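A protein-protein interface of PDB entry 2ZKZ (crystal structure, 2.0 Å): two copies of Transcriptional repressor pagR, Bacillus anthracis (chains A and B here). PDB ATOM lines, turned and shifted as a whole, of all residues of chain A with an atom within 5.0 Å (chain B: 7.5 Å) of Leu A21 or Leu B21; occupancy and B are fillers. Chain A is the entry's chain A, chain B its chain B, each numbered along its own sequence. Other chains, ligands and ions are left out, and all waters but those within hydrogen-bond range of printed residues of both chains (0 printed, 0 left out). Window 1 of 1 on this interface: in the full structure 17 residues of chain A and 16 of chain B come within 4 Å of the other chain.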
ATOM      1  N   ASP A  17       4.598   3.381  -7.275  1.00  0.00           N
ATOM      2  CA  ASP A  17       4.845   4.609  -6.520  1.00  0.00           C
ATOM      3  C   ASP A  17       6.220   4.588  -5.852  1.00  0.00           C
ATOM      4  O   ASP A  17       6.935   5.591  -5.866  1.00  0.00           O
ATOM      5  CB  ASP A  17       3.757   4.828  -5.466  1.00  0.00           C
ATOM      6  CG  ASP A  17       2.384   5.037  -6.084  1.00  0.00           C
ATOM      7  OD1 ASP A  17       2.306   5.611  -7.194  1.00  0.00           O
ATOM      8  OD2 ASP A  17       1.384   4.640  -5.450  1.00  0.00           O
ATOM      9  N   ALA A  18       6.590   3.457  -5.256  1.00  0.00           N
ATOM     10  CA  ALA A  18       7.902   3.327  -4.612  1.00  0.00           C
ATOM     11  C   ALA A  18       9.027   3.472  -5.639  1.00  0.00           C
ATOM     12  O   ALA A  18      10.042   4.135  -5.390  1.00  0.00           O
ATOM     13  CB  ALA A  18       8.016   1.969  -3.906  1.00  0.00           C
ATOM     14  N   GLU A  19       8.840   2.833  -6.790  1.00  0.00           N
ATOM     15  CA  GLU A  19       9.814   2.868  -7.878  1.00  0.00           C
ATOM     16  C   GLU A  19       9.938   4.287  -8.454  1.00  0.00           C
ATOM     17  O   GLU A  19      11.016   4.696  -8.879  1.00  0.00           O
ATOM     18  CB  GLU A  19       9.400   1.863  -8.970  1.00  0.00           C
ATOM     19  CG  GLU A  19      10.316   1.794 -10.196  1.00  0.00           C
ATOM     20  CD  GLU A  19      11.747   1.419  -9.854  1.00  0.00           C
ATOM     21  OE1 GLU A  19      11.986   0.915  -8.738  1.00  0.00           O
ATOM     22  OE2 GLU A  19      12.638   1.619 -10.708  1.00  0.00           O
ATOM     23  N   LEU A  20       8.839   5.035  -8.459  1.00  0.00           N
ATOM     24  CA  LEU A  20       8.848   6.414  -8.955  1.00  0.00           C
ATOM     25  C   LEU A  20       9.723   7.275  -8.044  1.00  0.00           C
ATOM     26  O   LEU A  20      10.545   8.061  -8.508  1.00  0.00           O
ATOM     27  CB  LEU A  20       7.426   7.000  -8.978  1.00  0.00           C
ATOM     28  CG  LEU A  20       7.259   8.385  -9.620  1.00  0.00           C
ATOM     29  CD1 LEU A  20       7.518   8.274 -11.131  1.00  0.00           C
ATOM     30  CD2 LEU A  20       5.854   8.914  -9.376  1.00  0.00           C
ATOM     31  N   LEU A  21       9.549   7.121  -6.738  1.00  0.00           N
ATOM     32  CA  LEU A  21      10.343   7.898  -5.797  1.00  0.00           C
ATOM     33  C   LEU A  21      11.810   7.486  -5.896  1.00  0.00           C
ATOM     34  O   LEU A  21      12.694   8.332  -5.863  1.00  0.00           O
ATOM     35  CB  LEU A  21       9.827   7.696  -4.367  1.00  0.00           C
ATOM     36  CG  LEU A  21       8.367   8.072  -4.085  1.00  0.00           C
ATOM     37  CD1 LEU A  21       8.079   7.868  -2.588  1.00  0.00           C
ATOM     38  CD2 LEU A  21       8.100   9.517  -4.476  1.00  0.00           C
ATOM     39  N   LYS A  22      12.065   6.188  -6.032  1.00  0.00           N
ATOM     40  CA  LYS A  22      13.435   5.699  -6.141  1.00  0.00           C
ATOM     41  C   LYS A  22      14.147   6.297  -7.358  1.00  0.00           C
ATOM     42  O   LYS A  22      15.298   6.719  -7.269  1.00  0.00           O
ATOM     43  CB  LYS A  22      13.448   4.175  -6.238  1.00  0.00           C
ATOM     44  CG  LYS A  22      14.850   3.567  -6.325  1.00  0.00           C
ATOM     45  CD  LYS A  22      14.786   2.077  -6.653  1.00  0.00           C
ATOM     46  CE  LYS A  22      16.175   1.470  -6.798  1.00  0.00           C
ATOM     47  NZ  LYS A  22      16.890   1.473  -5.493  1.00  0.00           N
ATOM     48  N   THR A  23      13.445   6.348  -8.489  1.00  0.00           N
ATOM     49  CA  THR A  23      14.011   6.881  -9.720  1.00  0.00           C
ATOM     50  C   THR A  23      14.302   8.379  -9.636  1.00  0.00           C
ATOM     51  O   THR A  23      15.233   8.867 -10.273  1.00  0.00           O
ATOM     52  CB  THR A  23      13.078   6.591 -10.927  1.00  0.00           C
ATOM     53  OG1 THR A  23      12.792   5.188 -10.974  1.00  0.00           O
ATOM     54  CG2 THR A  23      13.754   6.989 -12.247  1.00  0.00           C
ATOM     55  N   MET A  24      13.509   9.108  -8.855  1.00  0.00           N
ATOM     56  CA  MET A  24      13.707  10.555  -8.680  1.00  0.00           C
ATOM     57  C   MET A  24      14.664  10.877  -7.527  1.00  0.00           C
ATOM     58  O   MET A  24      15.078  12.026  -7.366  1.00  0.00           O
ATOM     59  CB  MET A  24      12.373  11.254  -8.365  1.00  0.00           C
ATOM     60  CG  MET A  24      11.263  11.126  -9.411  1.00  0.00           C
ATOM     61  SD  MET A  24       9.602  11.948  -8.780  1.00  0.00           S
ATOM     62  CE  MET A  24      10.184  13.788  -8.766  1.00  0.00           C
ATOM     63  N   ALA A  25      15.018   9.872  -6.731  1.00  0.00           N
ATOM     64  CA  ALA A  25      15.866  10.080  -5.555  1.00  0.00           C
ATOM     65  C   ALA A  25      17.356  10.363  -5.767  1.00  0.00           C
ATOM     66  O   ALA A  25      18.206   9.736  -5.140  1.00  0.00           O
ATOM     67  CB  ALA A  25      15.692   8.898  -4.585  1.00  0.00           C
ATOM     68  N   LEU A  30      16.507  15.395  -9.636  1.00  0.00           N
ATOM     69  CA  LEU A  30      15.482  16.327  -9.180  1.00  0.00           C
ATOM     70  C   LEU A  30      15.678  17.657  -9.916  1.00  0.00           C
ATOM     71  O   LEU A  30      14.710  18.334 -10.244  1.00  0.00           O
ATOM     72  CB  LEU A  30      15.557  16.520  -7.660  1.00  0.00           C
ATOM     73  CG  LEU A  30      15.094  15.300  -6.845  1.00  0.00           C
ATOM     74  CD1 LEU A  30      15.312  15.543  -5.347  1.00  0.00           C
ATOM     75  CD2 LEU A  30      13.617  15.031  -7.134  1.00  0.00           C
ATOM     76  N   ILE A  91       4.906  16.194  -7.270  1.00  0.00           N
ATOM     77  CA  ILE A  91       6.004  16.042  -6.328  1.00  0.00           C
ATOM     78  C   ILE A  91       7.055  17.125  -6.463  1.00  0.00           C
ATOM     79  O   ILE A  91       7.532  17.658  -5.460  1.00  0.00           O
ATOM     80  CB  ILE A  91       6.709  14.668  -6.479  1.00  0.00           C
ATOM     81  CG1 ILE A  91       5.755  13.538  -6.088  1.00  0.00           C
ATOM     82  CG2 ILE A  91       7.949  14.619  -5.589  1.00  0.00           C
ATOM     83  CD1 ILE A  91       6.275  12.148  -6.425  1.00  0.00           C
ATOM     84  N   LEU A  95       8.270  19.940  -3.620  1.00  0.00           N
ATOM     85  CA  LEU A  95       9.653  19.988  -3.173  1.00  0.00           C
ATOM     86  C   LEU A  95      10.309  21.359  -3.238  1.00  0.00           C
ATOM     87  O   LEU A  95      11.271  21.616  -2.508  1.00  0.00           O
ATOM     88  CB  LEU A  95      10.492  18.974  -3.952  1.00  0.00           C
ATOM     89  CG  LEU A  95      10.166  17.508  -3.654  1.00  0.00           C
ATOM     90  CD1 LEU A  95      11.052  16.597  -4.492  1.00  0.00           C
ATOM     91  CD2 LEU A  95      10.371  17.236  -2.164  1.00  0.00           C
ATOM     92  N   LEU B  14      18.492  20.071  -2.479  1.00  0.00           N
ATOM     93  CA  LEU B  14      18.321  18.984  -3.432  1.00  0.00           C
ATOM     94  C   LEU B  14      18.768  17.660  -2.831  1.00  0.00           C
ATOM     95  O   LEU B  14      18.141  16.635  -3.064  1.00  0.00           O
ATOM     96  CB  LEU B  14      19.123  19.253  -4.706  1.00  0.00           C
ATOM     97  CG  LEU B  14      18.489  20.214  -5.709  1.00  0.00           C
ATOM     98  CD1 LEU B  14      19.533  20.652  -6.726  1.00  0.00           C
ATOM     99  CD2 LEU B  14      17.312  19.528  -6.391  1.00  0.00           C
ATOM    100  N   GLU B  15      19.852  17.689  -2.063  1.00  0.00           N
ATOM    101  CA  GLU B  15      20.367  16.473  -1.447  1.00  0.00           C
ATOM    102  C   GLU B  15      19.405  16.000  -0.367  1.00  0.00           C
ATOM    103  O   GLU B  15      19.132  14.801  -0.252  1.00  0.00           O
ATOM    104  CB  GLU B  15      21.744  16.714  -0.829  1.00  0.00           C
ATOM    105  CG  GLU B  15      22.715  15.572  -1.066  1.00  0.00           C
ATOM    106  CD  GLU B  15      22.151  14.214  -0.664  1.00  0.00           C
ATOM    107  OE1 GLU B  15      21.994  13.960   0.551  1.00  0.00           O
ATOM    108  OE2 GLU B  15      21.865  13.398  -1.569  1.00  0.00           O
ATOM    109  N   ASP B  16      18.912  16.954   0.424  1.00  0.00           N
ATOM    110  CA  ASP B  16      17.954  16.676   1.494  1.00  0.00           C
ATOM    111  C   ASP B  16      16.737  16.004   0.882  1.00  0.00           C
ATOM    112  O   ASP B  16      16.275  14.969   1.365  1.00  0.00           O
ATOM    113  CB  ASP B  16      17.489  17.977   2.164  1.00  0.00           C
ATOM    114  CG  ASP B  16      18.508  18.548   3.135  1.00  0.00           C
ATOM    115  OD1 ASP B  16      18.424  19.766   3.416  1.00  0.00           O
ATOM    116  OD2 ASP B  16      19.372  17.792   3.632  1.00  0.00           O
ATOM    117  N   ASP B  17      16.211  16.611  -0.179  1.00  0.00           N
ATOM    118  CA  ASP B  17      15.034  16.076  -0.846  1.00  0.00           C
ATOM    119  C   ASP B  17      15.274  14.714  -1.471  1.00  0.00           C
ATOM    120  O   ASP B  17      14.406  13.849  -1.416  1.00  0.00           O
ATOM    121  CB  ASP B  17      14.526  17.047  -1.914  1.00  0.00           C
ATOM    122  CG  ASP B  17      14.100  18.380  -1.329  1.00  0.00           C
ATOM    123  OD1 ASP B  17      13.950  18.459  -0.089  1.00  0.00           O
ATOM    124  OD2 ASP B  17      13.912  19.342  -2.107  1.00  0.00           O
ATOM    125  N   ALA B  18      16.447  14.525  -2.064  1.00  0.00           N
ATOM    126  CA  ALA B  18      16.775  13.244  -2.682  1.00  0.00           C
ATOM    127  C   ALA B  18      16.825  12.144  -1.627  1.00  0.00           C
ATOM    128  O   ALA B  18      16.334  11.038  -1.853  1.00  0.00           O
ATOM    129  CB  ALA B  18      18.111  13.336  -3.408  1.00  0.00           C
ATOM    130  N   GLU B  19      17.418  12.445  -0.474  1.00  0.00           N
ATOM    131  CA  GLU B  19      17.518  11.454   0.596  1.00  0.00           C
ATOM    132  C   GLU B  19      16.143  11.134   1.188  1.00  0.00           C
ATOM    133  O   GLU B  19      15.876  10.003   1.601  1.00  0.00           O
ATOM    134  CB  GLU B  19      18.463  11.952   1.694  1.00  0.00           C
ATOM    135  CG  GLU B  19      18.864  10.873   2.691  1.00  0.00           C
ATOM    136  CD  GLU B  19      19.434   9.633   2.011  1.00  0.00           C
ATOM    137  OE1 GLU B  19      20.325   9.779   1.143  1.00  0.00           O
ATOM    138  OE2 GLU B  19      18.995   8.513   2.349  1.00  0.00           O
ATOM    139  N   LEU B  20      15.269  12.131   1.226  1.00  0.00           N
ATOM    140  CA  LEU B  20      13.921  11.934   1.745  1.00  0.00           C
ATOM    141  C   LEU B  20      13.204  10.910   0.852  1.00  0.00           C
ATOM    142  O   LEU B  20      12.608   9.944   1.336  1.00  0.00           O
ATOM    143  CB  LEU B  20      13.162  13.259   1.728  1.00  0.00           C
ATOM    144  CG  LEU B  20      11.830  13.306   2.469  1.00  0.00           C
ATOM    145  CD1 LEU B  20      12.110  13.318   3.976  1.00  0.00           C
ATOM    146  CD2 LEU B  20      11.061  14.559   2.076  1.00  0.00           C
ATOM    147  N   LEU B  21      13.264  11.131  -0.459  1.00  0.00           N
ATOM    148  CA  LEU B  21      12.638  10.225  -1.427  1.00  0.00           C
ATOM    149  C   LEU B  21      13.243   8.823  -1.354  1.00  0.00           C
ATOM    150  O   LEU B  21      12.529   7.817  -1.402  1.00  0.00           O
ATOM    151  CB  LEU B  21      12.810  10.782  -2.851  1.00  0.00           C
ATOM    152  CG  LEU B  21      11.677  11.609  -3.488  1.00  0.00           C
ATOM    153  CD1 LEU B  21      11.009  12.497  -2.476  1.00  0.00           C
ATOM    154  CD2 LEU B  21      12.238  12.434  -4.642  1.00  0.00           C
ATOM    155  N   LYS B  22      14.565   8.759  -1.235  1.00  0.00           N
ATOM    156  CA  LYS B  22      15.263   7.482  -1.177  1.00  0.00           C
ATOM    157  C   LYS B  22      14.772   6.658   0.016  1.00  0.00           C
ATOM    158  O   LYS B  22      14.494   5.470  -0.102  1.00  0.00           O
ATOM    159  CB  LYS B  22      16.770   7.737  -1.064  1.00  0.00           C
ATOM    160  CG  LYS B  22      17.650   6.500  -1.187  1.00  0.00           C
ATOM    161  CD  LYS B  22      19.124   6.909  -1.291  1.00  0.00           C
ATOM    162  CE  LYS B  22      20.043   5.711  -1.533  1.00  0.00           C
ATOM    163  NZ  LYS B  22      20.137   4.811  -0.346  1.00  0.00           N
ATOM    164  N   THR B  23      14.641   7.317   1.160  1.00  0.00           N
ATOM    165  CA  THR B  23      14.197   6.660   2.373  1.00  0.00           C
ATOM    166  C   THR B  23      12.756   6.172   2.267  1.00  0.00           C
ATOM    167  O   THR B  23      12.412   5.131   2.824  1.00  0.00           O
ATOM    168  CB  THR B  23      14.356   7.613   3.569  1.00  0.00           C
ATOM    169  OG1 THR B  23      15.721   8.054   3.624  1.00  0.00           O
ATOM    170  CG2 THR B  23      13.993   6.914   4.882  1.00  0.00           C
ATOM    171  N   MET B  24      11.919   6.913   1.544  1.00  0.00           N
ATOM    172  CA  MET B  24      10.515   6.539   1.363  1.00  0.00           C
ATOM    173  C   MET B  24      10.303   5.506   0.254  1.00  0.00           C
ATOM    174  O   MET B  24       9.264   4.853   0.203  1.00  0.00           O
ATOM    175  CB  MET B  24       9.669   7.767   0.982  1.00  0.00           C
ATOM    176  CG  MET B  24       9.588   8.891   2.015  1.00  0.00           C
ATOM    177  SD  MET B  24       8.578  10.391   1.261  1.00  0.00           S
ATOM    178  CE  MET B  24       6.836   9.573   1.182  1.00  0.00           C
ATOM    179  N   ALA B  25      11.282   5.376  -0.634  1.00  0.00           N
ATOM    180  CA  ALA B  25      11.187   4.500  -1.807  1.00  0.00           C
ATOM    181  C   ALA B  25      11.129   2.983  -1.649  1.00  0.00           C
ATOM    182  O   ALA B  25      11.875   2.265  -2.308  1.00  0.00           O
ATOM    183  CB  ALA B  25      12.300   4.865  -2.792  1.00  0.00           C
ATOM    184  N   HIS B  26      10.219   2.499  -0.810  1.00  0.00           N
ATOM    185  CA  HIS B  26      10.034   1.065  -0.581  1.00  0.00           C
ATOM    186  C   HIS B  26       8.544   0.874  -0.352  1.00  0.00           C
ATOM    187  O   HIS B  26       7.926   1.637   0.387  1.00  0.00           O
ATOM    188  CB  HIS B  26      10.809   0.610   0.659  1.00  0.00           C
ATOM    189  CG  HIS B  26      12.291   0.758   0.524  1.00  0.00           C
ATOM    190  ND1 HIS B  26      13.086  -0.208  -0.053  1.00  0.00           N
ATOM    191  CD2 HIS B  26      13.118   1.778   0.853  1.00  0.00           C
ATOM    192  CE1 HIS B  26      14.339   0.209  -0.071  1.00  0.00           C
ATOM    193  NE2 HIS B  26      14.386   1.411   0.473  1.00  0.00           N
ATOM    194  N   ARG B  29       7.326   0.780   3.244  1.00  0.00           N
ATOM    195  CA  ARG B  29       7.596   2.028   3.931  1.00  0.00           C
ATOM    196  C   ARG B  29       6.518   3.025   3.549  1.00  0.00           C
ATOM    197  O   ARG B  29       6.081   3.813   4.379  1.00  0.00           O
ATOM    198  CB  ARG B  29       8.979   2.557   3.567  1.00  0.00           C
ATOM    199  CG  ARG B  29      10.096   1.615   3.997  1.00  0.00           C
ATOM    200  CD  ARG B  29      11.430   2.301   3.940  1.00  0.00           C
ATOM    201  NE  ARG B  29      12.527   1.378   4.200  1.00  0.00           N
ATOM    202  CZ  ARG B  29      13.809   1.710   4.098  1.00  0.00           C
ATOM    203  NH1 ARG B  29      14.142   2.943   3.742  1.00  0.00           N
ATOM    204  NH2 ARG B  29      14.751   0.817   4.355  1.00  0.00           N
ATOM    205  N   LEU B  30       6.077   2.989   2.293  1.00  0.00           N
ATOM    206  CA  LEU B  30       5.017   3.890   1.870  1.00  0.00           C
ATOM    207  C   LEU B  30       3.729   3.496   2.577  1.00  0.00           C
ATOM    208  O   LEU B  30       2.916   4.346   2.929  1.00  0.00           O
ATOM    209  CB  LEU B  30       4.810   3.824   0.353  1.00  0.00           C
ATOM    210  CG  LEU B  30       5.872   4.516  -0.501  1.00  0.00           C
ATOM    211  CD1 LEU B  30       5.527   4.350  -1.986  1.00  0.00           C
ATOM    212  CD2 LEU B  30       5.931   5.991  -0.136  1.00  0.00           C
ATOM    213  N   VAL B  69      12.459  10.879   7.908  1.00  0.00           N
ATOM    214  CA  VAL B  69      11.081  10.680   7.476  1.00  0.00           C
ATOM    215  C   VAL B  69      10.096  10.635   8.644  1.00  0.00           C
ATOM    216  O   VAL B  69       9.011  11.222   8.578  1.00  0.00           O
ATOM    217  CB  VAL B  69      10.956   9.381   6.634  1.00  0.00           C
ATOM    218  CG1 VAL B  69       9.500   9.048   6.382  1.00  0.00           C
ATOM    219  CG2 VAL B  69      11.687   9.560   5.308  1.00  0.00           C
ATOM    220  N   LYS B  87       6.908  17.747   3.883  1.00  0.00           N
ATOM    221  CA  LYS B  87       7.102  17.234   2.526  1.00  0.00           C
ATOM    222  C   LYS B  87       6.631  15.781   2.412  1.00  0.00           C
ATOM    223  O   LYS B  87       6.055  15.381   1.403  1.00  0.00           O
ATOM    224  CB  LYS B  87       8.580  17.312   2.132  1.00  0.00           C
ATOM    225  CG  LYS B  87       9.126  18.722   1.890  1.00  0.00           C
ATOM    226  CD  LYS B  87      10.629  18.663   1.632  1.00  0.00           C
ATOM    227  CE  LYS B  87      11.183  19.980   1.084  1.00  0.00           C
ATOM    228  NZ  LYS B  87      10.927  21.124   1.986  1.00  0.00           N
ATOM    229  N   VAL B  88       6.900  14.994   3.449  1.00  0.00           N
ATOM    230  CA  VAL B  88       6.511  13.586   3.475  1.00  0.00           C
ATOM    231  C   VAL B  88       4.995  13.452   3.398  1.00  0.00           C
ATOM    232  O   VAL B  88       4.462  12.637   2.648  1.00  0.00           O
ATOM    233  CB  VAL B  88       7.013  12.898   4.776  1.00  0.00           C
ATOM    234  CG1 VAL B  88       6.517  11.446   4.838  1.00  0.00           C
ATOM    235  CG2 VAL B  88       8.527  12.950   4.831  1.00  0.00           C
ATOM    236  N   ILE B  91       3.719  14.407  -0.077  1.00  0.00           N
ATOM    237  CA  ILE B  91       3.982  13.347  -1.055  1.00  0.00           C
ATOM    238  C   ILE B  91       3.033  12.162  -0.896  1.00  0.00           C
ATOM    239  O   ILE B  91       2.490  11.654  -1.880  1.00  0.00           O
ATOM    240  CB  ILE B  91       5.444  12.840  -0.947  1.00  0.00           C
ATOM    241  CG1 ILE B  91       6.403  13.910  -1.476  1.00  0.00           C
ATOM    242  CG2 ILE B  91       5.616  11.527  -1.721  1.00  0.00           C
ATOM    243  CD1 ILE B  91       7.835  13.706  -1.060  1.00  0.00           C
ATOM    244  N   ILE B  92       2.829  11.720   0.340  1.00  0.00           N
ATOM    245  CA  ILE B  92       1.944  10.590   0.593  1.00  0.00           C
ATOM    246  C   ILE B  92       0.521  10.900   0.106  1.00  0.00           C
ATOM    247  O   ILE B  92      -0.133  10.045  -0.504  1.00  0.00           O
ATOM    248  CB  ILE B  92       1.955  10.199   2.111  1.00  0.00           C
ATOM    249  CG1 ILE B  92       2.283   8.712   2.254  1.00  0.00           C
ATOM    250  CG2 ILE B  92       0.620  10.510   2.774  1.00  0.00           C
ATOM    251  CD1 ILE B  92       1.362   7.788   1.502  1.00  0.00           C
ATOM    252  N   LEU B  95       0.305  10.610  -3.654  1.00  0.00           N
ATOM    253  CA  LEU B  95       0.375   9.228  -4.115  1.00  0.00           C
ATOM    254  C   LEU B  95      -0.865   8.369  -3.864  1.00  0.00           C
ATOM    255  O   LEU B  95      -1.087   7.384  -4.572  1.00  0.00           O
ATOM    256  CB  LEU B  95       1.596   8.530  -3.504  1.00  0.00           C
ATOM    257  CG  LEU B  95       2.976   9.063  -3.893  1.00  0.00           C
ATOM    258  CD1 LEU B  95       4.046   8.227  -3.212  1.00  0.00           C
ATOM    259  CD2 LEU B  95       3.151   9.009  -5.408  1.00  0.00           C
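Leu B30 touches Asp A17.
Asp A17 touches Leu B95 (OD2 to O, 3.8 Å).
Ala B25 touches Ala A18.
CB of Met B24 touches CD1 of Leu A21, at 3.9 Å.
CB of Met A24 touches CD2 of Leu B21 (3.9 Å).
CB of Leu B21 touches CB of Ala A25 (3.9 Å).
N of Lys B22 touches CB of Ala A25, at 3.5 Å.
Leu B14 touches Leu A30.
Leu B21 touches Leu A30 (CD2 to CD2, 3.9 Å).
O of Leu A95 touches CE of Lys B87 (3.9 Å).
Of the 12 printed residues of chain A, 8 touch a printed residue of chain B.
Of the 21 printed residues of chain B, 11 touch a printed residue of chain A.
Hydrophobic or aromatic side chains of chain B that line the printed part of chain A: Leu B14, Ala B18, Leu B21, Met B24, Ala B25, Leu B30 and Leu B95.
Among the printed residues, no Asp or Glu carboxylate lies within 4 Å of a Lys or Arg side-chain nitrogen of the other chain.
Asp A17 touches Leu B30, and with the chains exchanged Leu A30 touches Asp B17.
Ala A18 touches Leu B30, and with the chains exchanged Leu A30 touches Ala B18.
Leu A21 touches its own counterpart, Leu B21.
Leu A21 touches Met B24, and with the chains exchanged Met A24 touches Leu B21.
Positions printed for both chains: 17, 18, 19, 20, 21, 22, 23, 24, 25, 30, 91 and 95.
Of the 19 pairs that touch across the chains among the printed residues, 15 have their exchanged pair printed and touching as well.
Leu A21 touches just these residues of chain B: Leu B21, Met B24 and Leu B30.
Of chain A, only Leu A21 (3.9 Å), Met A24 (3.9 Å), Ala A25 (3.9 Å) and Leu A30 (3.9 Å) come within 4 Å of Leu B21.
Of the printed residues of chain B, Asp A17 touches Leu B30 (3.9 Å) and Leu B95 (3.8 Å).
Printed residues of chain B within 4 Å of Leu A30: Leu B14, Asp B17, Ala B18 and Leu B21.
Printed residues of chain B within 4 Å of Ala A25: Ala B18, Leu B21 and Lys B22.
Of the printed residues of chain B, Ala A18 touches Ala B25, His B26 and Leu B30.
Thr B23 touches none of the printed residues of chain A.
The nearest printed residue of chain A that does not touch Lys B22 is Leu A21 (5.0 Å).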
